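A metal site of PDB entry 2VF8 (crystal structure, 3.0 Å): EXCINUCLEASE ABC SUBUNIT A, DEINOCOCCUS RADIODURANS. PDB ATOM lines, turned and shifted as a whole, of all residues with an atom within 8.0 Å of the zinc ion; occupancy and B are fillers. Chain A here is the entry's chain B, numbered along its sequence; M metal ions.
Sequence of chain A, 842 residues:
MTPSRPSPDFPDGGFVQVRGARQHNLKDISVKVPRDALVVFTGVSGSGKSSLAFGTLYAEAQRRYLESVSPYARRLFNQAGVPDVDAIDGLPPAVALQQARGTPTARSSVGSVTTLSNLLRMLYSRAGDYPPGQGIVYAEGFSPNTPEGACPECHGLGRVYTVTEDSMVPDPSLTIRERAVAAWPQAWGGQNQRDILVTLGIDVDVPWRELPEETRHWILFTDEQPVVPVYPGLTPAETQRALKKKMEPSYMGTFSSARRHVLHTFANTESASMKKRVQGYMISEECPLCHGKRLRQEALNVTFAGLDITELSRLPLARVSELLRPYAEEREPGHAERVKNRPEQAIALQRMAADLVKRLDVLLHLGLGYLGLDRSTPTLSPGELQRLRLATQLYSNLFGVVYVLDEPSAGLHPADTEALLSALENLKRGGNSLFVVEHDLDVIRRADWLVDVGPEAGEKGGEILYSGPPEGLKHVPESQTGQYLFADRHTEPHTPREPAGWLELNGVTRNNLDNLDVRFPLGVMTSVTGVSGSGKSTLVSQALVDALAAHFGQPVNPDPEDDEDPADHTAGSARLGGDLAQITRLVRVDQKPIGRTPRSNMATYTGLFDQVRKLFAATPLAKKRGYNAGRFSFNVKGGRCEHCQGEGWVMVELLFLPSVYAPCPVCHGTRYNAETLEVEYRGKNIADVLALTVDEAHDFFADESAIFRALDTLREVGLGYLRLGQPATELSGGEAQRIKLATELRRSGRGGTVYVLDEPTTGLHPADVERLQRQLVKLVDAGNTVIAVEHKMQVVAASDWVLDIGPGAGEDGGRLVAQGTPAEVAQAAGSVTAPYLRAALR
The side-chain sulfur of Cys 644 lies close to the backbone NH of Gly 646 (3.5 Å).
The backbone carbonyl oxygen of Cys 641 is in hydrogen-bond range of the backbone NH of Gly 646 (3.2 Å).
The backbone NH (N) of Gly 648 lies close to the side-chain sulfur (SG) of Cys 644 (3.2 Å).
The side-chain sulfur of Cys 641 sits close to the backbone NH of His 643 (3.5 Å).
The side-chain sulfur (SG) of Cys 667 lies close to the backbone NH (N) of Arg 671 (3.4 Å).
The backbone NH (N) of Cys 641 lies within hydrogen-bond range of the backbone carbonyl oxygen (O) of Arg 671 (2.7 Å).
The backbone NH of Val 666 sits close to the side-chain sulfur of Cys 664 (3.6 Å).
The backbone NH of Cys 664 lies within hydrogen-bond range of the backbone carbonyl oxygen of Gly 648 (2.9 Å).
Of the 22 residues printed, 4 come within 4 Å of the zinc ion.
The nearest printed residue that does not touch the zinc ion is His 643 (4.3 Å).
The zinc ion is bound by SG of Cys 667 (2.2 Å), SG of Cys 664 (2.2 Å), SG of Cys 644 (2.4 Å) and SG of Cys 641 (2.5 Å).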
ATOM      1  N   ARG A 640     -26.125   0.798   9.278  1.00  0.00           N
ATOM      2  CA  ARG A 640     -24.671   0.874   9.297  1.00  0.00           C
ATOM      3  C   ARG A 640     -24.202   2.189   9.929  1.00  0.00           C
ATOM      4  O   ARG A 640     -24.950   3.192   9.924  1.00  0.00           O
ATOM      5  CB  ARG A 640     -24.116   0.718   7.879  1.00  0.00           C
ATOM      6  CG  ARG A 640     -23.855   2.001   7.101  1.00  0.00           C
ATOM      7  CD  ARG A 640     -23.263   1.721   5.705  1.00  0.00           C
ATOM      8  NE  ARG A 640     -22.580   2.865   5.108  1.00  0.00           N
ATOM      9  CZ  ARG A 640     -22.295   3.005   3.811  1.00  0.00           C
ATOM     10  NH1 ARG A 640     -22.628   2.080   2.929  1.00  0.00           N
ATOM     11  NH2 ARG A 640     -21.663   4.088   3.389  1.00  0.00           N
ATOM     12  N   CYS A 641     -23.004   2.180  10.487  1.00  0.00           N
ATOM     13  CA  CYS A 641     -22.350   3.413  10.947  1.00  0.00           C
ATOM     14  C   CYS A 641     -21.777   4.189   9.743  1.00  0.00           C
ATOM     15  O   CYS A 641     -21.405   3.592   8.751  1.00  0.00           O
ATOM     16  CB  CYS A 641     -21.247   3.070  11.939  1.00  0.00           C
ATOM     17  SG  CYS A 641     -19.918   4.256  12.004  1.00  0.00           S
ATOM     18  N   GLU A 642     -21.702   5.514   9.825  1.00  0.00           N
ATOM     19  CA  GLU A 642     -21.320   6.277   8.638  1.00  0.00           C
ATOM     20  C   GLU A 642     -19.986   6.970   8.738  1.00  0.00           C
ATOM     21  O   GLU A 642     -19.485   7.501   7.750  1.00  0.00           O
ATOM     22  CB  GLU A 642     -22.379   7.309   8.267  1.00  0.00           C
ATOM     23  CG  GLU A 642     -23.779   6.775   8.083  1.00  0.00           C
ATOM     24  CD  GLU A 642     -23.953   5.972   6.799  1.00  0.00           C
ATOM     25  OE1 GLU A 642     -23.215   6.216   5.817  1.00  0.00           O
ATOM     26  OE2 GLU A 642     -24.866   5.103   6.801  1.00  0.00           O
ATOM     27  N   HIS A 643     -19.412   7.006   9.934  1.00  0.00           N
ATOM     28  CA  HIS A 643     -18.131   7.669  10.112  1.00  0.00           C
ATOM     29  C   HIS A 643     -17.017   6.952   9.350  1.00  0.00           C
ATOM     30  O   HIS A 643     -16.077   7.593   8.886  1.00  0.00           O
ATOM     31  CB  HIS A 643     -17.770   7.783  11.604  1.00  0.00           C
ATOM     32  CG  HIS A 643     -16.493   8.525  11.882  1.00  0.00           C
ATOM     33  ND1 HIS A 643     -16.457   9.740  12.526  1.00  0.00           N
ATOM     34  CD2 HIS A 643     -15.201   8.211  11.598  1.00  0.00           C
ATOM     35  CE1 HIS A 643     -15.202  10.143  12.648  1.00  0.00           C
ATOM     36  NE2 HIS A 643     -14.422   9.232  12.087  1.00  0.00           N
ATOM     37  N   CYS A 644     -17.148   5.632   9.232  1.00  0.00           N
ATOM     38  CA  CYS A 644     -16.167   4.775   8.539  1.00  0.00           C
ATOM     39  C   CYS A 644     -16.782   4.356   7.230  1.00  0.00           C
ATOM     40  O   CYS A 644     -16.093   4.191   6.223  1.00  0.00           O
ATOM     41  CB  CYS A 644     -15.852   3.521   9.364  1.00  0.00           C
ATOM     42  SG  CYS A 644     -17.291   2.609  10.001  1.00  0.00           S
ATOM     43  N   GLN A 645     -18.098   4.184   7.295  1.00  0.00           N
ATOM     44  CA  GLN A 645     -18.966   3.858   6.174  1.00  0.00           C
ATOM     45  C   GLN A 645     -19.318   2.387   6.116  1.00  0.00           C
ATOM     46  O   GLN A 645     -19.631   1.857   5.054  1.00  0.00           O
ATOM     47  CB  GLN A 645     -18.394   4.347   4.845  1.00  0.00           C
ATOM     48  CG  GLN A 645     -18.511   5.834   4.666  1.00  0.00           C
ATOM     49  CD  GLN A 645     -18.257   6.257   3.248  1.00  0.00           C
ATOM     50  OE1 GLN A 645     -19.054   5.970   2.346  1.00  0.00           O
ATOM     51  NE2 GLN A 645     -17.137   6.939   3.018  1.00  0.00           N
ATOM     52  N   GLY A 646     -19.287   1.735   7.274  1.00  0.00           N
ATOM     53  CA  GLY A 646     -19.611   0.318   7.380  1.00  0.00           C
ATOM     54  C   GLY A 646     -18.368  -0.528   7.311  1.00  0.00           C
ATOM     55  O   GLY A 646     -18.376  -1.688   7.682  1.00  0.00           O
ATOM     56  N   GLU A 647     -17.279   0.081   6.852  1.00  0.00           N
ATOM     57  CA  GLU A 647     -16.006  -0.589   6.820  1.00  0.00           C
ATOM     58  C   GLU A 647     -15.508  -0.935   8.224  1.00  0.00           C
ATOM     59  O   GLU A 647     -14.668  -1.803   8.366  1.00  0.00           O
ATOM     60  CB  GLU A 647     -14.957   0.260   6.097  1.00  0.00           C
ATOM     61  CG  GLU A 647     -15.003   0.149   4.579  1.00  0.00           C
ATOM     62  CD  GLU A 647     -13.981   1.032   3.896  1.00  0.00           C
ATOM     63  OE1 GLU A 647     -14.293   1.541   2.805  1.00  0.00           O
ATOM     64  OE2 GLU A 647     -12.867   1.229   4.432  1.00  0.00           O
ATOM     65  N   GLY A 648     -16.015  -0.241   9.234  1.00  0.00           N
ATOM     66  CA  GLY A 648     -15.585  -0.431  10.625  1.00  0.00           C
ATOM     67  C   GLY A 648     -14.160   0.008  10.920  1.00  0.00           C
ATOM     68  O   GLY A 648     -13.706  -0.108  12.059  1.00  0.00           O
ATOM     69  N   TRP A 649     -13.457   0.518   9.906  1.00  0.00           N
ATOM     70  CA  TRP A 649     -12.024   0.804   9.983  1.00  0.00           C
ATOM     71  C   TRP A 649     -11.616   2.035   9.154  1.00  0.00           C
ATOM     72  O   TRP A 649     -12.196   2.316   8.110  1.00  0.00           O
ATOM     73  CB  TRP A 649     -11.230  -0.456   9.581  1.00  0.00           C
ATOM     74  CG  TRP A 649     -11.513  -1.656  10.471  1.00  0.00           C
ATOM     75  CD1 TRP A 649     -12.666  -2.396  10.505  1.00  0.00           C
ATOM     76  CD2 TRP A 649     -10.644  -2.228  11.446  1.00  0.00           C
ATOM     77  NE1 TRP A 649     -12.564  -3.377  11.463  1.00  0.00           N
ATOM     78  CE2 TRP A 649     -11.333  -3.295  12.049  1.00  0.00           C
ATOM     79  CE3 TRP A 649      -9.349  -1.922  11.883  1.00  0.00           C
ATOM     80  CZ2 TRP A 649     -10.778  -4.064  13.050  1.00  0.00           C
ATOM     81  CZ3 TRP A 649      -8.803  -2.691  12.894  1.00  0.00           C
ATOM     82  CH2 TRP A 649      -9.516  -3.753  13.459  1.00  0.00           C
ATOM     83  N   VAL A 650     -10.598   2.750   9.635  1.00  0.00           N
ATOM     84  CA  VAL A 650     -10.127   3.988   9.040  1.00  0.00           C
ATOM     85  C   VAL A 650      -8.632   3.876   8.851  1.00  0.00           C
ATOM     86  O   VAL A 650      -7.976   3.183   9.617  1.00  0.00           O
ATOM     87  CB  VAL A 650     -10.389   5.151   9.976  1.00  0.00           C
ATOM     88  CG1 VAL A 650     -10.133   6.481   9.290  1.00  0.00           C
ATOM     89  CG2 VAL A 650     -11.808   5.108  10.485  1.00  0.00           C
ATOM     90  N   PRO A 663      -9.093   0.754  14.097  1.00  0.00           N
ATOM     91  CA  PRO A 663     -10.527   0.644  14.326  1.00  0.00           C
ATOM     92  C   PRO A 663     -11.218   1.989  14.228  1.00  0.00           C
ATOM     93  O   PRO A 663     -10.689   2.992  14.706  1.00  0.00           O
ATOM     94  CB  PRO A 663     -10.634   0.114  15.753  1.00  0.00           C
ATOM     95  CG  PRO A 663      -9.369  -0.555  15.998  1.00  0.00           C
ATOM     96  CD  PRO A 663      -8.335   0.199  15.236  1.00  0.00           C
ATOM     97  N   CYS A 664     -12.383   2.001  13.598  1.00  0.00           N
ATOM     98  CA  CYS A 664     -13.184   3.201  13.505  1.00  0.00           C
ATOM     99  C   CYS A 664     -13.373   3.752  14.897  1.00  0.00           C
ATOM    100  O   CYS A 664     -13.760   3.015  15.802  1.00  0.00           O
ATOM    101  CB  CYS A 664     -14.533   2.879  12.924  1.00  0.00           C
ATOM    102  SG  CYS A 664     -15.559   4.280  12.806  1.00  0.00           S
ATOM    103  N   PRO A 665     -13.083   5.046  15.083  1.00  0.00           N
ATOM    104  CA  PRO A 665     -13.208   5.736  16.370  1.00  0.00           C
ATOM    105  C   PRO A 665     -14.642   5.881  16.880  1.00  0.00           C
ATOM    106  O   PRO A 665     -14.846   5.859  18.096  1.00  0.00           O
ATOM    107  CB  PRO A 665     -12.615   7.107  16.084  1.00  0.00           C
ATOM    108  CG  PRO A 665     -12.760   7.288  14.625  1.00  0.00           C
ATOM    109  CD  PRO A 665     -12.545   5.942  14.041  1.00  0.00           C
ATOM    110  N   VAL A 666     -15.612   6.041  15.984  1.00  0.00           N
ATOM    111  CA  VAL A 666     -17.006   6.263  16.365  1.00  0.00           C
ATOM    112  C   VAL A 666     -17.669   4.955  16.781  1.00  0.00           C
ATOM    113  O   VAL A 666     -18.098   4.820  17.923  1.00  0.00           O
ATOM    114  CB  VAL A 666     -17.827   6.943  15.247  1.00  0.00           C
ATOM    115  CG1 VAL A 666     -19.318   6.758  15.463  1.00  0.00           C
ATOM    116  CG2 VAL A 666     -17.516   8.397  15.190  1.00  0.00           C
ATOM    117  N   CYS A 667     -17.759   4.008  15.860  1.00  0.00           N
ATOM    118  CA  CYS A 667     -18.523   2.807  16.131  1.00  0.00           C
ATOM    119  C   CYS A 667     -17.687   1.699  16.775  1.00  0.00           C
ATOM    120  O   CYS A 667     -18.225   0.817  17.431  1.00  0.00           O
ATOM    121  CB  CYS A 667     -19.220   2.310  14.870  1.00  0.00           C
ATOM    122  SG  CYS A 667     -18.121   1.856  13.573  1.00  0.00           S
ATOM    123  N   HIS A 668     -16.365   1.782  16.556  1.00  0.00           N
ATOM    124  CA  HIS A 668     -15.349   0.961  17.233  1.00  0.00           C
ATOM    125  C   HIS A 668     -15.134  -0.418  16.652  1.00  0.00           C
ATOM    126  O   HIS A 668     -15.114  -1.397  17.369  1.00  0.00           O
ATOM    127  CB  HIS A 668     -15.591   0.871  18.744  1.00  0.00           C
ATOM    128  CG  HIS A 668     -15.435   2.176  19.432  1.00  0.00           C
ATOM    129  ND1 HIS A 668     -14.223   2.809  19.556  1.00  0.00           N
ATOM    130  CD2 HIS A 668     -16.349   2.986  20.029  1.00  0.00           C
ATOM    131  CE1 HIS A 668     -14.389   3.955  20.196  1.00  0.00           C
ATOM    132  NE2 HIS A 668     -15.673   4.092  20.491  1.00  0.00           N
ATOM    133  N   GLY A 669     -14.931  -0.461  15.339  1.00  0.00           N
ATOM    134  CA  GLY A 669     -14.671  -1.730  14.667  1.00  0.00           C
ATOM    135  C   GLY A 669     -15.935  -2.541  14.497  1.00  0.00           C
ATOM    136  O   GLY A 669     -15.881  -3.668  14.011  1.00  0.00           O
ATOM    137  N   THR A 670     -17.062  -1.947  14.874  1.00  0.00           N
ATOM    138  CA  THR A 670     -18.334  -2.640  14.935  1.00  0.00           C
ATOM    139  C   THR A 670     -19.138  -2.568  13.652  1.00  0.00           C
ATOM    140  O   THR A 670     -19.683  -3.575  13.225  1.00  0.00           O
ATOM    141  CB  THR A 670     -19.147  -2.180  16.136  1.00  0.00           C
ATOM    142  OG1 THR A 670     -19.706  -3.324  16.788  1.00  0.00           O
ATOM    143  CG2 THR A 670     -20.244  -1.164  15.753  1.00  0.00           C
ATOM    144  N   ARG A 671     -19.214  -1.359  13.070  1.00  0.00           N
ATOM    145  CA  ARG A 671     -19.745  -1.062  11.699  1.00  0.00           C
ATOM    146  C   ARG A 671     -21.157  -0.502  11.663  1.00  0.00           C
ATOM    147  O   ARG A 671     -21.712  -0.238  10.603  1.00  0.00           O
ATOM    148  CB  ARG A 671     -19.608  -2.242  10.745  1.00  0.00           C
ATOM    149  CG  ARG A 671     -18.193  -2.803  10.729  1.00  0.00           C
ATOM    150  CD  ARG A 671     -18.122  -4.161  10.129  1.00  0.00           C
ATOM    151  NE  ARG A 671     -17.352  -4.116   8.898  1.00  0.00           N
ATOM    152  CZ  ARG A 671     -16.739  -5.172   8.386  1.00  0.00           C
ATOM    153  NH1 ARG A 671     -16.828  -6.322   9.010  1.00  0.00           N
ATOM    154  NH2 ARG A 671     -16.043  -5.067   7.254  1.00  0.00           N
ATOM    155  N   TYR A 672     -21.703  -0.262  12.853  1.00  0.00           N
ATOM    156  CA  TYR A 672     -23.136  -0.112  13.016  1.00  0.00           C
ATOM    157  C   TYR A 672     -23.583   0.973  14.016  1.00  0.00           C
ATOM    158  O   TYR A 672     -23.055   1.059  15.144  1.00  0.00           O
ATOM    159  CB  TYR A 672     -23.710  -1.473  13.435  1.00  0.00           C
ATOM    160  CG  TYR A 672     -23.810  -2.456  12.282  1.00  0.00           C
ATOM    161  CD1 TYR A 672     -24.761  -2.260  11.280  1.00  0.00           C
ATOM    162  CD2 TYR A 672     -22.967  -3.561  12.208  1.00  0.00           C
ATOM    163  CE1 TYR A 672     -24.879  -3.136  10.212  1.00  0.00           C
ATOM    164  CE2 TYR A 672     -23.082  -4.459  11.136  1.00  0.00           C
ATOM    165  CZ  TYR A 672     -24.043  -4.229  10.142  1.00  0.00           C
ATOM    166  OH  TYR A 672     -24.199  -5.058   9.066  1.00  0.00           O
ATOM    167  N   ASN A 673     -24.573   1.773  13.611  1.00  0.00           N
ATOM    168  CA  ASN A 673     -25.170   2.721  14.528  1.00  0.00           C
ATOM    169  C   ASN A 673     -25.941   2.018  15.657  1.00  0.00           C
ATOM    170  O   ASN A 673     -26.644   1.038  15.419  1.00  0.00           O
ATOM    171  CB  ASN A 673     -25.928   3.871  13.807  1.00  0.00           C
ATOM    172  CG  ASN A 673     -27.335   3.496  13.320  1.00  0.00           C
ATOM    173  OD1 ASN A 673     -27.961   2.524  13.766  1.00  0.00           O
ATOM    174  ND2 ASN A 673     -27.855   4.313  12.400  1.00  0.00           N
HETATM  175 ZN    ZN M   1     -17.562   3.508  12.213  1.00  0.00          ZN
